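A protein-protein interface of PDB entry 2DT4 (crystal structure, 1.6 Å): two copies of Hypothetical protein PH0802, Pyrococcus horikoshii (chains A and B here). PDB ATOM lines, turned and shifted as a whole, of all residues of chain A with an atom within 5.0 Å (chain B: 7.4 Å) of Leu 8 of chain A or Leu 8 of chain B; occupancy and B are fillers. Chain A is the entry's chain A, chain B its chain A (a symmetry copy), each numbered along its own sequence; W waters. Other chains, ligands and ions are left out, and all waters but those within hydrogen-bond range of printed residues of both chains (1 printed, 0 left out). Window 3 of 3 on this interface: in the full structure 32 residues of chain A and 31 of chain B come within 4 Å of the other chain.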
ATOM      1  N   PHE A   6     -10.184  21.569 -12.773  1.00  0.00           N
ATOM      2  CA  PHE A   6     -10.513  22.062 -11.443  1.00  0.00           C
ATOM      3  C   PHE A   6     -10.995  20.930 -10.549  1.00  0.00           C
ATOM      4  O   PHE A   6     -11.439  19.880 -11.020  1.00  0.00           O
ATOM      5  CB  PHE A   6     -11.633  23.115 -11.520  1.00  0.00           C
ATOM      6  CG  PHE A   6     -11.266  24.300 -12.320  1.00  0.00           C
ATOM      7  CD1 PHE A   6     -10.592  25.358 -11.733  1.00  0.00           C
ATOM      8  CD2 PHE A   6     -11.494  24.331 -13.684  1.00  0.00           C
ATOM      9  CE1 PHE A   6     -10.207  26.442 -12.496  1.00  0.00           C
ATOM     10  CE2 PHE A   6     -11.108  25.406 -14.444  1.00  0.00           C
ATOM     11  CZ  PHE A   6     -10.440  26.467 -13.840  1.00  0.00           C
ATOM     12  N   SER A   7     -10.929  21.166  -9.246  1.00  0.00           N
ATOM     13  CA  SER A   7     -11.532  20.267  -8.293  1.00  0.00           C
ATOM     14  C   SER A   7     -12.921  20.770  -7.933  1.00  0.00           C
ATOM     15  O   SER A   7     -13.252  21.970  -8.062  1.00  0.00           O
ATOM     16  CB  SER A   7     -10.686  20.112  -7.015  1.00  0.00           C
ATOM     17  OG  SER A   7     -10.530  21.324  -6.330  1.00  0.00           O
ATOM     18  N   LEU A   8     -13.742  19.858  -7.452  1.00  0.00           N
ATOM     19  CA  LEU A   8     -15.121  20.212  -7.096  1.00  0.00           C
ATOM     20  C   LEU A   8     -15.112  20.791  -5.684  1.00  0.00           C
ATOM     21  O   LEU A   8     -14.727  20.111  -4.718  1.00  0.00           O
ATOM     22  CB  LEU A   8     -16.044  18.988  -7.183  1.00  0.00           C
ATOM     23  CG  LEU A   8     -16.280  18.486  -8.592  1.00  0.00           C
ATOM     24  CD1 LEU A   8     -16.763  17.001  -8.561  1.00  0.00           C
ATOM     25  CD2 LEU A   8     -17.296  19.379  -9.341  1.00  0.00           C
ATOM     26  N   GLY A   9     -15.500  22.049  -5.576  1.00  0.00           N
ATOM     27  CA  GLY A   9     -15.708  22.682  -4.296  1.00  0.00           C
ATOM     28  C   GLY A   9     -17.100  22.494  -3.767  1.00  0.00           C
ATOM     29  O   GLY A   9     -17.722  21.447  -3.971  1.00  0.00           O
ATOM     30  N   ARG A  10     -17.588  23.524  -3.089  1.00  0.00           N
ATOM     31  CA  ARG A  10     -18.886  23.500  -2.446  1.00  0.00           C
ATOM     32  C   ARG A  10     -19.991  23.444  -3.489  1.00  0.00           C
ATOM     33  O   ARG A  10     -19.852  23.992  -4.589  1.00  0.00           O
ATOM     34  CB  ARG A  10     -19.045  24.703  -1.511  1.00  0.00           C
ATOM     35  CG  ARG A  10     -18.095  24.639  -0.319  1.00  0.00           C
ATOM     36  CD  ARG A  10     -17.970  25.930   0.422  1.00  0.00           C
ATOM     37  NE  ARG A  10     -17.245  26.927  -0.350  1.00  0.00           N
ATOM     38  CZ  ARG A  10     -17.194  28.240  -0.105  1.00  0.00           C
ATOM     39  NH1 ARG A  10     -16.454  29.012  -0.912  1.00  0.00           N
ATOM     40  NH2 ARG A  10     -17.856  28.768   0.912  1.00  0.00           N
ATOM     41  N   THR A  11     -21.063  22.770  -3.116  1.00  0.00           N
ATOM     42  CA  THR A  11     -22.216  22.509  -3.983  1.00  0.00           C
ATOM     43  C   THR A  11     -23.492  23.084  -3.332  1.00  0.00           C
ATOM     44  O   THR A  11     -23.705  22.932  -2.131  1.00  0.00           O
ATOM     45  CB  THR A  11     -22.356  20.998  -4.164  1.00  0.00           C
ATOM     46  OG1 THR A  11     -21.123  20.447  -4.664  1.00  0.00           O
ATOM     47  CG2 THR A  11     -23.438  20.680  -5.181  1.00  0.00           C
ATOM     48  N   GLN A 119     -22.196  25.059  -8.529  1.00  0.00           N
ATOM     49  CA  GLN A 119     -21.087  24.173  -8.197  1.00  0.00           C
ATOM     50  C   GLN A 119     -19.804  24.980  -8.261  1.00  0.00           C
ATOM     51  O   GLN A 119     -19.347  25.374  -9.349  1.00  0.00           O
ATOM     52  CB  GLN A 119     -21.023  22.960  -9.154  1.00  0.00           C
ATOM     53  CG  GLN A 119     -19.787  22.082  -8.968  1.00  0.00           C
ATOM     54  CD  GLN A 119     -19.771  21.477  -7.565  1.00  0.00           C
ATOM     55  OE1 GLN A 119     -18.873  21.793  -6.741  1.00  0.00           O
ATOM     56  NE2 GLN A 119     -20.754  20.666  -7.269  1.00  0.00           N
ATOM     57  N   GLU A 120     -19.192  25.151  -7.092  1.00  0.00           N
ATOM     58  CA  GLU A 120     -17.928  25.857  -7.010  1.00  0.00           C
ATOM     59  C   GLU A 120     -16.827  24.984  -7.582  1.00  0.00           C
ATOM     60  O   GLU A 120     -16.870  23.770  -7.416  1.00  0.00           O
ATOM     61  CB  GLU A 120     -17.613  26.163  -5.533  1.00  0.00           C
ATOM     62  CG  GLU A 120     -16.273  26.804  -5.291  1.00  0.00           C
ATOM     63  CD  GLU A 120     -15.964  27.000  -3.834  1.00  0.00           C
ATOM     64  OE1 GLU A 120     -15.328  28.038  -3.531  1.00  0.00           O
ATOM     65  OE2 GLU A 120     -16.333  26.131  -3.007  1.00  0.00           O
ATOM     66  N   LEU A 121     -15.865  25.614  -8.255  1.00  0.00           N
ATOM     67  CA  LEU A 121     -14.674  24.947  -8.787  1.00  0.00           C
ATOM     68  C   LEU A 121     -13.423  25.588  -8.198  1.00  0.00           C
ATOM     69  O   LEU A 121     -13.381  26.816  -8.025  1.00  0.00           O
ATOM     70  CB  LEU A 121     -14.643  25.124 -10.296  1.00  0.00           C
ATOM     71  CG  LEU A 121     -15.824  24.522 -11.065  1.00  0.00           C
ATOM     72  CD1 LEU A 121     -15.646  24.744 -12.556  1.00  0.00           C
ATOM     73  CD2 LEU A 121     -16.090  23.029 -10.755  1.00  0.00           C
ATOM     74  N   LYS A 122     -12.435  24.748  -7.849  1.00  0.00           N
ATOM     75  CA  LYS A 122     -11.215  25.183  -7.180  1.00  0.00           C
ATOM     76  C   LYS A 122     -10.029  24.801  -8.050  1.00  0.00           C
ATOM     77  O   LYS A 122      -9.945  23.706  -8.584  1.00  0.00           O
ATOM     78  CB  LYS A 122     -11.051  24.499  -5.818  1.00  0.00           C
ATOM     79  CG  LYS A 122     -12.212  24.610  -4.838  1.00  0.00           C
ATOM     80  CD  LYS A 122     -12.270  25.952  -4.241  1.00  0.00           C
ATOM     81  CE  LYS A 122     -12.846  25.890  -2.830  1.00  0.00           C
ATOM     82  NZ  LYS A 122     -12.976  27.174  -2.152  1.00  0.00           N
ATOM     83  N   PHE B   6     -24.970  21.491   0.060  1.00  0.00           N
ATOM     84  CA  PHE B   6     -25.127  20.044   0.051  1.00  0.00           C
ATOM     85  C   PHE B   6     -23.825  19.360  -0.335  1.00  0.00           C
ATOM     86  O   PHE B   6     -22.940  19.958  -0.953  1.00  0.00           O
ATOM     87  CB  PHE B   6     -26.202  19.625  -0.967  1.00  0.00           C
ATOM     88  CG  PHE B   6     -27.536  20.183  -0.670  1.00  0.00           C
ATOM     89  CD1 PHE B   6     -28.393  19.524   0.198  1.00  0.00           C
ATOM     90  CD2 PHE B   6     -27.914  21.418  -1.166  1.00  0.00           C
ATOM     91  CE1 PHE B   6     -29.618  20.074   0.512  1.00  0.00           C
ATOM     92  CE2 PHE B   6     -29.130  21.968  -0.852  1.00  0.00           C
ATOM     93  CZ  PHE B   6     -29.985  21.290   0.014  1.00  0.00           C
ATOM     94  N   SER B   7     -23.726  18.084   0.014  1.00  0.00           N
ATOM     95  CA  SER B   7     -22.640  17.263  -0.459  1.00  0.00           C
ATOM     96  C   SER B   7     -23.083  16.501  -1.697  1.00  0.00           C
ATOM     97  O   SER B   7     -24.287  16.268  -1.943  1.00  0.00           O
ATOM     98  CB  SER B   7     -22.143  16.274   0.614  1.00  0.00           C
ATOM     99  OG  SER B   7     -23.141  15.372   1.007  1.00  0.00           O
ATOM    100  N   LEU B   8     -22.108  16.082  -2.479  1.00  0.00           N
ATOM    101  CA  LEU B   8     -22.408  15.362  -3.721  1.00  0.00           C
ATOM    102  C   LEU B   8     -22.616  13.889  -3.377  1.00  0.00           C
ATOM    103  O   LEU B   8     -21.705  13.218  -2.863  1.00  0.00           O
ATOM    104  CB  LEU B   8     -21.276  15.532  -4.744  1.00  0.00           C
ATOM    105  CG  LEU B   8     -21.149  16.934  -5.302  1.00  0.00           C
ATOM    106  CD1 LEU B   8     -19.718  17.149  -5.895  1.00  0.00           C
ATOM    107  CD2 LEU B   8     -22.233  17.211  -6.369  1.00  0.00           C
ATOM    108  N   GLY B   9     -23.821  13.406  -3.625  1.00  0.00           N
ATOM    109  CA  GLY B   9     -24.121  12.000  -3.515  1.00  0.00           C
ATOM    110  C   GLY B   9     -23.854  11.240  -4.781  1.00  0.00           C
ATOM    111  O   GLY B   9     -22.912  11.544  -5.519  1.00  0.00           O
ATOM    112  N   ARG B  10     -24.699  10.249  -5.031  1.00  0.00           N
ATOM    113  CA  ARG B  10     -24.559   9.363  -6.170  1.00  0.00           C
ATOM    114  C   ARG B  10     -24.801  10.124  -7.464  1.00  0.00           C
ATOM    115  O   ARG B  10     -25.600  11.066  -7.505  1.00  0.00           O
ATOM    116  CB  ARG B  10     -25.496   8.159  -6.031  1.00  0.00           C
ATOM    117  CG  ARG B  10     -25.105   7.251  -4.869  1.00  0.00           C
ATOM    118  CD  ARG B  10     -26.167   6.272  -4.486  1.00  0.00           C
ATOM    119  NE  ARG B  10     -27.299   6.925  -3.851  1.00  0.00           N
ATOM    120  CZ  ARG B  10     -28.508   6.395  -3.639  1.00  0.00           C
ATOM    121  NH1 ARG B  10     -29.431   7.138  -3.014  1.00  0.00           N
ATOM    122  NH2 ARG B  10     -28.788   5.162  -4.033  1.00  0.00           N
ATOM    123  N   THR B  11     -24.091   9.696  -8.491  1.00  0.00           N
ATOM    124  CA  THR B  11     -24.092  10.328  -9.814  1.00  0.00           C
ATOM    125  C   THR B  11     -24.530   9.298 -10.878  1.00  0.00           C
ATOM    126  O   THR B  11     -24.091   8.150 -10.855  1.00  0.00           O
ATOM    127  CB  THR B  11     -22.680  10.826 -10.117  1.00  0.00           C
ATOM    128  OG1 THR B  11     -22.230  11.697  -9.063  1.00  0.00           O
ATOM    129  CG2 THR B  11     -22.662  11.628 -11.406  1.00  0.00           C
ATOM    130  N   ILE B  39     -30.320  17.004  -8.911  1.00  0.00           N
ATOM    131  CA  ILE B  39     -30.404  17.956 -10.005  1.00  0.00           C
ATOM    132  C   ILE B  39     -30.347  17.055 -11.232  1.00  0.00           C
ATOM    133  O   ILE B  39     -29.741  15.968 -11.225  1.00  0.00           O
ATOM    134  CB  ILE B  39     -29.412  19.140 -10.074  1.00  0.00           C
ATOM    135  CG1 ILE B  39     -27.944  18.657 -10.062  1.00  0.00           C
ATOM    136  CG2 ILE B  39     -29.716  20.085  -8.931  1.00  0.00           C
ATOM    137  CD1 ILE B  39     -27.351  18.387 -11.410  1.00  0.00           C
ATOM    138  N   GLN B 119     -27.692  14.036 -10.498  1.00  0.00           N
ATOM    139  CA  GLN B 119     -26.715  14.172  -9.425  1.00  0.00           C
ATOM    140  C   GLN B 119     -27.469  14.321  -8.117  1.00  0.00           C
ATOM    141  O   GLN B 119     -28.106  15.357  -7.858  1.00  0.00           O
ATOM    142  CB  GLN B 119     -25.776  15.379  -9.661  1.00  0.00           C
ATOM    143  CG  GLN B 119     -24.839  15.678  -8.492  1.00  0.00           C
ATOM    144  CD  GLN B 119     -23.904  14.496  -8.244  1.00  0.00           C
ATOM    145  OE1 GLN B 119     -23.975  13.837  -7.174  1.00  0.00           O
ATOM    146  NE2 GLN B 119     -23.077  14.193  -9.213  1.00  0.00           N
ATOM    147  N   GLU B 120     -27.323  13.308  -7.269  1.00  0.00           N
ATOM    148  CA  GLU B 120     -27.945  13.337  -5.958  1.00  0.00           C
ATOM    149  C   GLU B 120     -27.205  14.324  -5.075  1.00  0.00           C
ATOM    150  O   GLU B 120     -25.990  14.444  -5.187  1.00  0.00           O
ATOM    151  CB  GLU B 120     -27.862  11.935  -5.326  1.00  0.00           C
ATOM    152  CG  GLU B 120     -28.378  11.846  -3.914  1.00  0.00           C
ATOM    153  CD  GLU B 120     -28.195  10.487  -3.301  1.00  0.00           C
ATOM    154  OE1 GLU B 120     -29.103  10.094  -2.530  1.00  0.00           O
ATOM    155  OE2 GLU B 120     -27.160   9.828  -3.568  1.00  0.00           O
ATOM    156  N   LEU B 121     -27.949  15.023  -4.219  1.00  0.00           N
ATOM    157  CA  LEU B 121     -27.397  15.943  -3.222  1.00  0.00           C
ATOM    158  C   LEU B 121     -27.830  15.505  -1.827  1.00  0.00           C
ATOM    159  O   LEU B 121     -28.973  15.061  -1.647  1.00  0.00           O
ATOM    160  CB  LEU B 121     -27.942  17.337  -3.483  1.00  0.00           C
ATOM    161  CG  LEU B 121     -27.592  17.950  -4.842  1.00  0.00           C
ATOM    162  CD1 LEU B 121     -28.170  19.349  -4.952  1.00  0.00           C
ATOM    163  CD2 LEU B 121     -26.078  17.951  -5.166  1.00  0.00           C
ATOM    164  N   LYS B 122     -26.896  15.589  -0.865  1.00  0.00           N
ATOM    165  CA  LYS B 122     -27.110  15.118   0.498  1.00  0.00           C
ATOM    166  C   LYS B 122     -26.918  16.289   1.446  1.00  0.00           C
ATOM    167  O   LYS B 122     -25.988  17.072   1.326  1.00  0.00           O
ATOM    168  CB  LYS B 122     -26.104  14.024   0.875  1.00  0.00           C
ATOM    169  CG  LYS B 122     -26.006  12.818  -0.049  1.00  0.00           C
ATOM    170  CD  LYS B 122     -27.158  11.924   0.130  1.00  0.00           C
ATOM    171  CE  LYS B 122     -26.767  10.476  -0.151  1.00  0.00           C
ATOM    172  NZ  LYS B 122     -27.845   9.502  -0.030  1.00  0.00           N
HETATM  173  O   HOH W   1     -20.655  21.105  -0.649  1.00  0.00           O
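Of the 10 printed residues of chain A, 3 touch a printed residue of chain B.
Hydrophobic or aromatic side chains of chain B that line the printed part of chain A: Leu 8 and Leu 121.
Among the printed residues, 5 pairs touch across the chains.
The backbone carbonyl oxygen (O) of Gly 9 of chain A sits close to the side-chain amide oxygen (OE1) of Gln 119 of chain A (3.0 Å).
OE1 of Gln 119 of chain A sits close to O of Arg 10 of chain A, 3.2 Å away.
The side-chain hydroxyl of Thr 11 of chain A lies within hydrogen-bond range of the side-chain amide nitrogen of Gln 119 of chain A (2.6 Å).
Among the printed residues, merely in contact across the chains: Thr 11 of chain A with Leu 8 of chain B (3.6 Å), Thr 11 of chain A with Leu 121 of chain B (3.8 Å), Gln 119 of chain A with Leu 8 of chain B (3.9 Å) and Leu 8 of chain A with Leu 8 of chain B (3.98 Å).
Of the printed residues of chain B, Leu 8 of chain A touches Leu 8 (3.98 Å).
Of the printed residues of chain A, Leu 8 of chain B touches Leu 8, Thr 11 and Gln 119.
No residue of chain B comes within 4 Å of Gly 9 of chain A.
Of the printed residues of chain B, Gln 119 of chain A touches Leu 8 (3.9 Å).
Printed residues of chain B within 4 Å of Thr 11 of chain A: Phe 6, Leu 8 and Leu 121.
Printed residues of chain A within 4 Å of Phe 6 of chain B: Thr 11 (2.9 Å).
Gln 119 of chain B touches none of the printed residues of chain A.
Ile 39 of chain B touches none of the printed residues of chain A.
The nearest printed residue of chain B that does not touch Leu 8 of chain A is Gln 119 of chain B (6.9 Å).
The nearest printed residue of chain A that does not touch Leu 8 of chain B is Gly 9 of chain A (5.1 Å).
The nearest printed residue of chain B that does not touch Thr 11 of chain A is Ser 7 of chain B (5.2 Å).
Water W1 bridges the backbone carbonyl oxygen of Phe 6 of chain B (2.6 Å) and the backbone NH of Thr 11 of chain A (3.0 Å).
The backbone NH of Phe 6 of chain B is in hydrogen-bond range of the backbone carbonyl oxygen of Thr 11 of chain A.
Leu 8 of chain A touches its own counterpart, Leu 8 of chain B.
Thr 11 of chain A touches Phe 6 of chain B, but with the chains exchanged Phe 6 of chain A does not touch Thr 11 of chain B (13.7 Å).
Thr 11 of chain A touches Leu 8 of chain B, but with the chains exchanged Leu 8 of chain A does not touch Thr 11 of chain B (7.6 Å).
Gln 119 of chain A touches Leu 8 of chain B, but with the chains exchanged Leu 8 of chain A does not touch Gln 119 of chain B (6.9 Å).
Positions printed for both chains: 6, 7, 8, 9, 10, 11, 119, 120, 121 and 122.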
